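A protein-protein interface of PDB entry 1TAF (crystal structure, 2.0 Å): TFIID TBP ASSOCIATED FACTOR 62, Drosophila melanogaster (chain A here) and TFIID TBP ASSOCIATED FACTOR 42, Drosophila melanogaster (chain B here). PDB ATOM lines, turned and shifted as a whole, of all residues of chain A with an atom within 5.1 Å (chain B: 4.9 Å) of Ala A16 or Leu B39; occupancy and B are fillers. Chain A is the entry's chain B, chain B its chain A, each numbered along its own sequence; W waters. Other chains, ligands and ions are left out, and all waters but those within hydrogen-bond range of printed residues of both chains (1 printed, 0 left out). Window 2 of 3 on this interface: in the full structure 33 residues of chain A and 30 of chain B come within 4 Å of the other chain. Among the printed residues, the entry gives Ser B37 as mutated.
The side-chain amino group (NZ) of Lys B43 is in hydrogen-bond range of the backbone carbonyl oxygen (O) of Val A21, at 3.1 Å.
The side-chain amino group of Lys A13 sits at hydrogen-bond distance from the backbone carbonyl oxygen of Leu A24, at 3.0 Å.
N of Val A21 sits at hydrogen-bond distance from O of Ala A16.
Val B35 touches Met A12.
Ile A15 touches Thr B36 (CG2 to CG2, 3.6 Å).
Ala A16 touches Leu B39 (CB to CD1, 3.8 Å).
Ile A19 touches Thr B36 (CG2 to CG2, 3.5 Å).
Val A21 touches Ile B54.
Leu A24 touches Leu B39.
Leu A24 touches Ile B54.
Leu A32 touches Ile B38.
CD1 of Leu A32 touches CD2 of Leu B39, at 3.4 Å.
Val B59 touches Leu A32.
Printed residues of chain B within 4 Å of Ile A15: Val B35 (3.7 Å) and Thr B36 (3.6 Å).
Of chain B, only Leu B39 (3.8 Å) comes within 4 Å of Ala A16.
Of the printed residues of chain B, Leu A24 touches Leu B39 (3.5 Å) and Ile B54 (3.7 Å).
Of the printed residues of chain A, Ile B38 touches Leu A32 (3.8 Å).
Of the printed residues of chain A, Val B59 touches Leu A32.
The nearest printed residue of chain B that does not touch Ala A16 is Val B35 (5.6 Å).
The nearest residue of chain A that does not touch Leu B39 is Val A21 (4.1 Å).
The nearest printed residue of chain B that does not touch Ile A15 is Leu B39 (4.7 Å).
Of the 13 printed residues of chain A, 7 touch a printed residue of chain B.
Hydrophobic or aromatic side chains of chain A that line the printed part of chain B: Met A12, Ile A15, Ala A16, Ile A19, Val A21, Leu A24 and Leu A32.
Hydrophobic or aromatic side chains of chain B that line the printed part of chain A: Val B35, Ile B38, Leu B39, Ile B54 and Val B59.
Among the printed residues, 12 pairs touch across the chains.
Among the printed residues, no Asp or Glu carboxylate lies within 4 Å of a Lys or Arg side-chain nitrogen of the other chain.
Water W1 lies within hydrogen-bond range of the backbone carbonyl oxygen of Val A21 (2.6 Å), the backbone NH of Ile B54 (3.1 Å) and the side-chain amino group of Lys B43 (3.4 Å).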
ATOM      1  N   MET A  12     -30.371 -21.578  -8.453  1.00  0.00           N
ATOM      2  CA  MET A  12     -30.503 -20.143  -8.726  1.00  0.00           C
ATOM      3  C   MET A  12     -29.550 -19.369  -7.828  1.00  0.00           C
ATOM      4  O   MET A  12     -29.033 -18.320  -8.205  1.00  0.00           O
ATOM      5  CB  MET A  12     -31.937 -19.668  -8.457  1.00  0.00           C
ATOM      6  CG  MET A  12     -33.019 -20.425  -9.210  1.00  0.00           C
ATOM      7  SD  MET A  12     -32.919 -20.236 -10.988  1.00  0.00           S
ATOM      8  CE  MET A  12     -32.025 -21.708 -11.458  1.00  0.00           C
ATOM      9  N   LYS A  13     -29.356 -19.888  -6.622  1.00  0.00           N
ATOM     10  CA  LYS A  13     -28.475 -19.276  -5.636  1.00  0.00           C
ATOM     11  C   LYS A  13     -27.012 -19.328  -6.107  1.00  0.00           C
ATOM     12  O   LYS A  13     -26.257 -18.354  -5.984  1.00  0.00           O
ATOM     13  CB  LYS A  13     -28.605 -20.023  -4.303  1.00  0.00           C
ATOM     14  CG  LYS A  13     -30.033 -20.346  -3.867  1.00  0.00           C
ATOM     15  CD  LYS A  13     -30.691 -19.165  -3.177  1.00  0.00           C
ATOM     16  CE  LYS A  13     -31.746 -19.649  -2.177  1.00  0.00           C
ATOM     17  NZ  LYS A  13     -32.458 -18.525  -1.495  1.00  0.00           N
ATOM     18  N   VAL A  14     -26.615 -20.482  -6.632  1.00  0.00           N
ATOM     19  CA  VAL A  14     -25.263 -20.679  -7.121  1.00  0.00           C
ATOM     20  C   VAL A  14     -24.999 -19.726  -8.262  1.00  0.00           C
ATOM     21  O   VAL A  14     -23.940 -19.124  -8.329  1.00  0.00           O
ATOM     22  CB  VAL A  14     -25.062 -22.119  -7.612  1.00  0.00           C
ATOM     23  CG1 VAL A  14     -23.720 -22.265  -8.324  1.00  0.00           C
ATOM     24  CG2 VAL A  14     -25.169 -23.074  -6.426  1.00  0.00           C
ATOM     25  N   ILE A  15     -25.961 -19.610  -9.172  1.00  0.00           N
ATOM     26  CA  ILE A  15     -25.824 -18.711 -10.310  1.00  0.00           C
ATOM     27  C   ILE A  15     -25.699 -17.256  -9.830  1.00  0.00           C
ATOM     28  O   ILE A  15     -24.862 -16.505 -10.330  1.00  0.00           O
ATOM     29  CB  ILE A  15     -27.011 -18.875 -11.297  1.00  0.00           C
ATOM     30  CG1 ILE A  15     -26.937 -20.244 -11.976  1.00  0.00           C
ATOM     31  CG2 ILE A  15     -26.998 -17.759 -12.340  1.00  0.00           C
ATOM     32  CD1 ILE A  15     -28.125 -20.550 -12.869  1.00  0.00           C
ATOM     33  N   ALA A  16     -26.488 -16.887  -8.825  1.00  0.00           N
ATOM     34  CA  ALA A  16     -26.460 -15.532  -8.279  1.00  0.00           C
ATOM     35  C   ALA A  16     -25.076 -15.170  -7.730  1.00  0.00           C
ATOM     36  O   ALA A  16     -24.591 -14.048  -7.938  1.00  0.00           O
ATOM     37  CB  ALA A  16     -27.513 -15.375  -7.194  1.00  0.00           C
ATOM     38  N   GLU A  17     -24.435 -16.121  -7.050  1.00  0.00           N
ATOM     39  CA  GLU A  17     -23.106 -15.883  -6.499  1.00  0.00           C
ATOM     40  C   GLU A  17     -22.063 -15.764  -7.583  1.00  0.00           C
ATOM     41  O   GLU A  17     -21.132 -14.975  -7.470  1.00  0.00           O
ATOM     42  CB  GLU A  17     -22.687 -17.009  -5.570  1.00  0.00           C
ATOM     43  CG  GLU A  17     -23.381 -17.023  -4.252  1.00  0.00           C
ATOM     44  CD  GLU A  17     -22.539 -17.693  -3.193  1.00  0.00           C
ATOM     45  OE1 GLU A  17     -21.985 -18.788  -3.472  1.00  0.00           O
ATOM     46  OE2 GLU A  17     -22.416 -17.110  -2.092  1.00  0.00           O
ATOM     47  N   SER A  18     -22.199 -16.575  -8.623  1.00  0.00           N
ATOM     48  CA  SER A  18     -21.247 -16.566  -9.723  1.00  0.00           C
ATOM     49  C   SER A  18     -21.229 -15.251 -10.484  1.00  0.00           C
ATOM     50  O   SER A  18     -20.258 -14.948 -11.172  1.00  0.00           O
ATOM     51  CB  SER A  18     -21.532 -17.725 -10.674  1.00  0.00           C
ATOM     52  OG  SER A  18     -21.440 -18.963  -9.979  1.00  0.00           O
ATOM     53  N   ILE A  19     -22.306 -14.478 -10.389  1.00  0.00           N
ATOM     54  CA  ILE A  19     -22.354 -13.208 -11.082  1.00  0.00           C
ATOM     55  C   ILE A  19     -22.292 -12.017 -10.142  1.00  0.00           C
ATOM     56  O   ILE A  19     -22.387 -10.872 -10.574  1.00  0.00           O
ATOM     57  CB  ILE A  19     -23.560 -13.098 -12.045  1.00  0.00           C
ATOM     58  CG1 ILE A  19     -24.886 -13.083 -11.271  1.00  0.00           C
ATOM     59  CG2 ILE A  19     -23.492 -14.226 -13.082  1.00  0.00           C
ATOM     60  CD1 ILE A  19     -26.118 -12.768 -12.140  1.00  0.00           C
ATOM     61  N   GLY A  20     -22.154 -12.290  -8.855  1.00  0.00           N
ATOM     62  CA  GLY A  20     -22.032 -11.211  -7.893  1.00  0.00           C
ATOM     63  C   GLY A  20     -23.232 -10.360  -7.533  1.00  0.00           C
ATOM     64  O   GLY A  20     -23.054  -9.257  -6.997  1.00  0.00           O
ATOM     65  N   VAL A  21     -24.447 -10.857  -7.764  1.00  0.00           N
ATOM     66  CA  VAL A  21     -25.638 -10.076  -7.413  1.00  0.00           C
ATOM     67  C   VAL A  21     -26.070 -10.248  -5.955  1.00  0.00           C
ATOM     68  O   VAL A  21     -27.060  -9.668  -5.532  1.00  0.00           O
ATOM     69  CB  VAL A  21     -26.846 -10.376  -8.338  1.00  0.00           C
ATOM     70  CG1 VAL A  21     -26.500 -10.024  -9.776  1.00  0.00           C
ATOM     71  CG2 VAL A  21     -27.298 -11.844  -8.201  1.00  0.00           C
ATOM     72  N   GLY A  22     -25.327 -11.037  -5.187  1.00  0.00           N
ATOM     73  CA  GLY A  22     -25.685 -11.233  -3.796  1.00  0.00           C
ATOM     74  C   GLY A  22     -26.704 -12.340  -3.577  1.00  0.00           C
ATOM     75  O   GLY A  22     -26.971 -13.152  -4.465  1.00  0.00           O
ATOM     76  N   LEU A  24     -30.369 -14.222  -2.672  1.00  0.00           N
ATOM     77  CA  LEU A  24     -31.730 -14.164  -3.177  1.00  0.00           C
ATOM     78  C   LEU A  24     -32.636 -14.623  -2.061  1.00  0.00           C
ATOM     79  O   LEU A  24     -32.287 -15.529  -1.304  1.00  0.00           O
ATOM     80  CB  LEU A  24     -31.959 -15.136  -4.333  1.00  0.00           C
ATOM     81  CG  LEU A  24     -31.042 -15.130  -5.538  1.00  0.00           C
ATOM     82  CD1 LEU A  24     -31.510 -16.197  -6.534  1.00  0.00           C
ATOM     83  CD2 LEU A  24     -31.061 -13.741  -6.152  1.00  0.00           C
ATOM     84  N   LEU A  32     -37.824 -17.936  -9.852  1.00  0.00           N
ATOM     85  CA  LEU A  32     -36.879 -18.033 -10.958  1.00  0.00           C
ATOM     86  C   LEU A  32     -36.660 -19.468 -11.419  1.00  0.00           C
ATOM     87  O   LEU A  32     -36.539 -19.721 -12.613  1.00  0.00           O
ATOM     88  CB  LEU A  32     -35.531 -17.430 -10.560  1.00  0.00           C
ATOM     89  CG  LEU A  32     -35.202 -16.018 -11.028  1.00  0.00           C
ATOM     90  CD1 LEU A  32     -33.855 -15.645 -10.485  1.00  0.00           C
ATOM     91  CD2 LEU A  32     -35.190 -15.952 -12.542  1.00  0.00           C
ATOM     92  N   VAL B  35     -31.301 -16.842 -16.219  1.00  0.00           N
ATOM     93  CA  VAL B  35     -31.263 -16.485 -14.814  1.00  0.00           C
ATOM     94  C   VAL B  35     -30.378 -15.264 -14.577  1.00  0.00           C
ATOM     95  O   VAL B  35     -30.775 -14.333 -13.889  1.00  0.00           O
ATOM     96  CB  VAL B  35     -30.810 -17.676 -13.962  1.00  0.00           C
ATOM     97  CG1 VAL B  35     -30.618 -17.261 -12.518  1.00  0.00           C
ATOM     98  CG2 VAL B  35     -31.844 -18.788 -14.054  1.00  0.00           C
ATOM     99  N   THR B  36     -29.204 -15.227 -15.188  1.00  0.00           N
ATOM    100  CA  THR B  36     -28.335 -14.075 -14.995  1.00  0.00           C
ATOM    101  C   THR B  36     -28.987 -12.800 -15.555  1.00  0.00           C
ATOM    102  O   THR B  36     -28.913 -11.737 -14.948  1.00  0.00           O
ATOM    103  CB  THR B  36     -26.946 -14.294 -15.627  1.00  0.00           C
ATOM    104  OG1 THR B  36     -27.097 -14.655 -16.997  1.00  0.00           O
ATOM    105  CG2 THR B  36     -26.203 -15.400 -14.918  1.00  0.00           C
ATOM    106  N   SER B  37     -29.670 -12.914 -16.686  1.00  0.00           N
ATOM    107  CA  SER B  37     -30.304 -11.753 -17.282  1.00  0.00           C
ATOM    108  C   SER B  37     -31.378 -11.171 -16.359  1.00  0.00           C
ATOM    109  O   SER B  37     -31.410  -9.968 -16.115  1.00  0.00           O
ATOM    110  CB  SER B  37     -30.903 -12.117 -18.631  1.00  0.00           C
ATOM    111  OG  SER B  37     -31.568 -10.999 -19.184  1.00  0.00           O
ATOM    112  N   ILE B  38     -32.241 -12.033 -15.829  1.00  0.00           N
ATOM    113  CA  ILE B  38     -33.297 -11.597 -14.927  1.00  0.00           C
ATOM    114  C   ILE B  38     -32.707 -11.018 -13.636  1.00  0.00           C
ATOM    115  O   ILE B  38     -33.138  -9.974 -13.181  1.00  0.00           O
ATOM    116  CB  ILE B  38     -34.231 -12.771 -14.561  1.00  0.00           C
ATOM    117  CG1 ILE B  38     -34.910 -13.333 -15.816  1.00  0.00           C
ATOM    118  CG2 ILE B  38     -35.246 -12.321 -13.506  1.00  0.00           C
ATOM    119  CD1 ILE B  38     -35.834 -12.343 -16.526  1.00  0.00           C
ATOM    120  N   LEU B  39     -31.710 -11.692 -13.066  1.00  0.00           N
ATOM    121  CA  LEU B  39     -31.079 -11.262 -11.807  1.00  0.00           C
ATOM    122  C   LEU B  39     -30.325  -9.958 -11.932  1.00  0.00           C
ATOM    123  O   LEU B  39     -30.307  -9.138 -11.019  1.00  0.00           O
ATOM    124  CB  LEU B  39     -30.143 -12.345 -11.267  1.00  0.00           C
ATOM    125  CG  LEU B  39     -30.810 -13.587 -10.676  1.00  0.00           C
ATOM    126  CD1 LEU B  39     -29.741 -14.571 -10.219  1.00  0.00           C
ATOM    127  CD2 LEU B  39     -31.708 -13.188  -9.513  1.00  0.00           C
ATOM    128  N   ASP B  40     -29.733  -9.753 -13.094  1.00  0.00           N
ATOM    129  CA  ASP B  40     -28.982  -8.543 -13.352  1.00  0.00           C
ATOM    130  C   ASP B  40     -29.886  -7.308 -13.279  1.00  0.00           C
ATOM    131  O   ASP B  40     -29.488  -6.268 -12.753  1.00  0.00           O
ATOM    132  CB  ASP B  40     -28.310  -8.666 -14.705  1.00  0.00           C
ATOM    133  CG  ASP B  40     -26.965  -8.043 -14.715  1.00  0.00           C
ATOM    134  OD1 ASP B  40     -26.099  -8.481 -13.933  1.00  0.00           O
ATOM    135  OD2 ASP B  40     -26.796  -7.088 -15.481  1.00  0.00           O
ATOM    136  N   ASP B  41     -31.107  -7.433 -13.796  1.00  0.00           N
ATOM    137  CA  ASP B  41     -32.078  -6.346 -13.757  1.00  0.00           C
ATOM    138  C   ASP B  41     -32.698  -6.239 -12.359  1.00  0.00           C
ATOM    139  O   ASP B  41     -32.884  -5.137 -11.818  1.00  0.00           O
ATOM    140  CB  ASP B  41     -33.180  -6.592 -14.789  1.00  0.00           C
ATOM    141  CG  ASP B  41     -32.676  -6.486 -16.219  1.00  0.00           C
ATOM    142  OD1 ASP B  41     -31.638  -5.849 -16.433  1.00  0.00           O
ATOM    143  OD2 ASP B  41     -33.320  -7.024 -17.130  1.00  0.00           O
ATOM    144  N   ALA B  42     -33.026  -7.393 -11.782  1.00  0.00           N
ATOM    145  CA  ALA B  42     -33.614  -7.448 -10.449  1.00  0.00           C
ATOM    146  C   ALA B  42     -32.699  -6.760  -9.427  1.00  0.00           C
ATOM    147  O   ALA B  42     -33.185  -6.118  -8.497  1.00  0.00           O
ATOM    148  CB  ALA B  42     -33.868  -8.896 -10.044  1.00  0.00           C
ATOM    149  N   LYS B  43     -31.384  -6.882  -9.608  1.00  0.00           N
ATOM    150  CA  LYS B  43     -30.415  -6.263  -8.700  1.00  0.00           C
ATOM    151  C   LYS B  43     -30.549  -4.739  -8.705  1.00  0.00           C
ATOM    152  O   LYS B  43     -30.438  -4.094  -7.667  1.00  0.00           O
ATOM    153  CB  LYS B  43     -28.982  -6.670  -9.074  1.00  0.00           C
ATOM    154  CG  LYS B  43     -27.894  -6.180  -8.086  1.00  0.00           C
ATOM    155  CD  LYS B  43     -28.208  -6.651  -6.660  1.00  0.00           C
ATOM    156  CE  LYS B  43     -27.133  -6.279  -5.636  1.00  0.00           C
ATOM    157  NZ  LYS B  43     -27.530  -6.828  -4.300  1.00  0.00           N
ATOM    158  N   ILE B  54     -32.193  -9.608  -3.153  1.00  0.00           N
ATOM    159  CA  ILE B  54     -33.167  -9.607  -4.242  1.00  0.00           C
ATOM    160  C   ILE B  54     -34.395 -10.367  -3.743  1.00  0.00           C
ATOM    161  O   ILE B  54     -34.268 -11.441  -3.165  1.00  0.00           O
ATOM    162  CB  ILE B  54     -32.586 -10.293  -5.521  1.00  0.00           C
ATOM    163  CG1 ILE B  54     -31.550  -9.371  -6.181  1.00  0.00           C
ATOM    164  CG2 ILE B  54     -33.690 -10.623  -6.521  1.00  0.00           C
ATOM    165  CD1 ILE B  54     -30.729 -10.060  -7.261  1.00  0.00           C
ATOM    166  N   VAL B  59     -37.680  -9.831  -8.971  1.00  0.00           N
ATOM    167  CA  VAL B  59     -37.665 -10.845 -10.030  1.00  0.00           C
ATOM    168  C   VAL B  59     -38.909 -10.696 -10.927  1.00  0.00           C
ATOM    169  O   VAL B  59     -38.824 -10.810 -12.150  1.00  0.00           O
ATOM    170  CB  VAL B  59     -37.610 -12.302  -9.438  1.00  0.00           C
ATOM    171  CG1 VAL B  59     -37.916 -13.325 -10.504  1.00  0.00           C
ATOM    172  CG2 VAL B  59     -36.237 -12.571  -8.848  1.00  0.00           C
HETATM  173  O   HOH W   1     -29.193  -9.727  -4.012  1.00  0.00           O
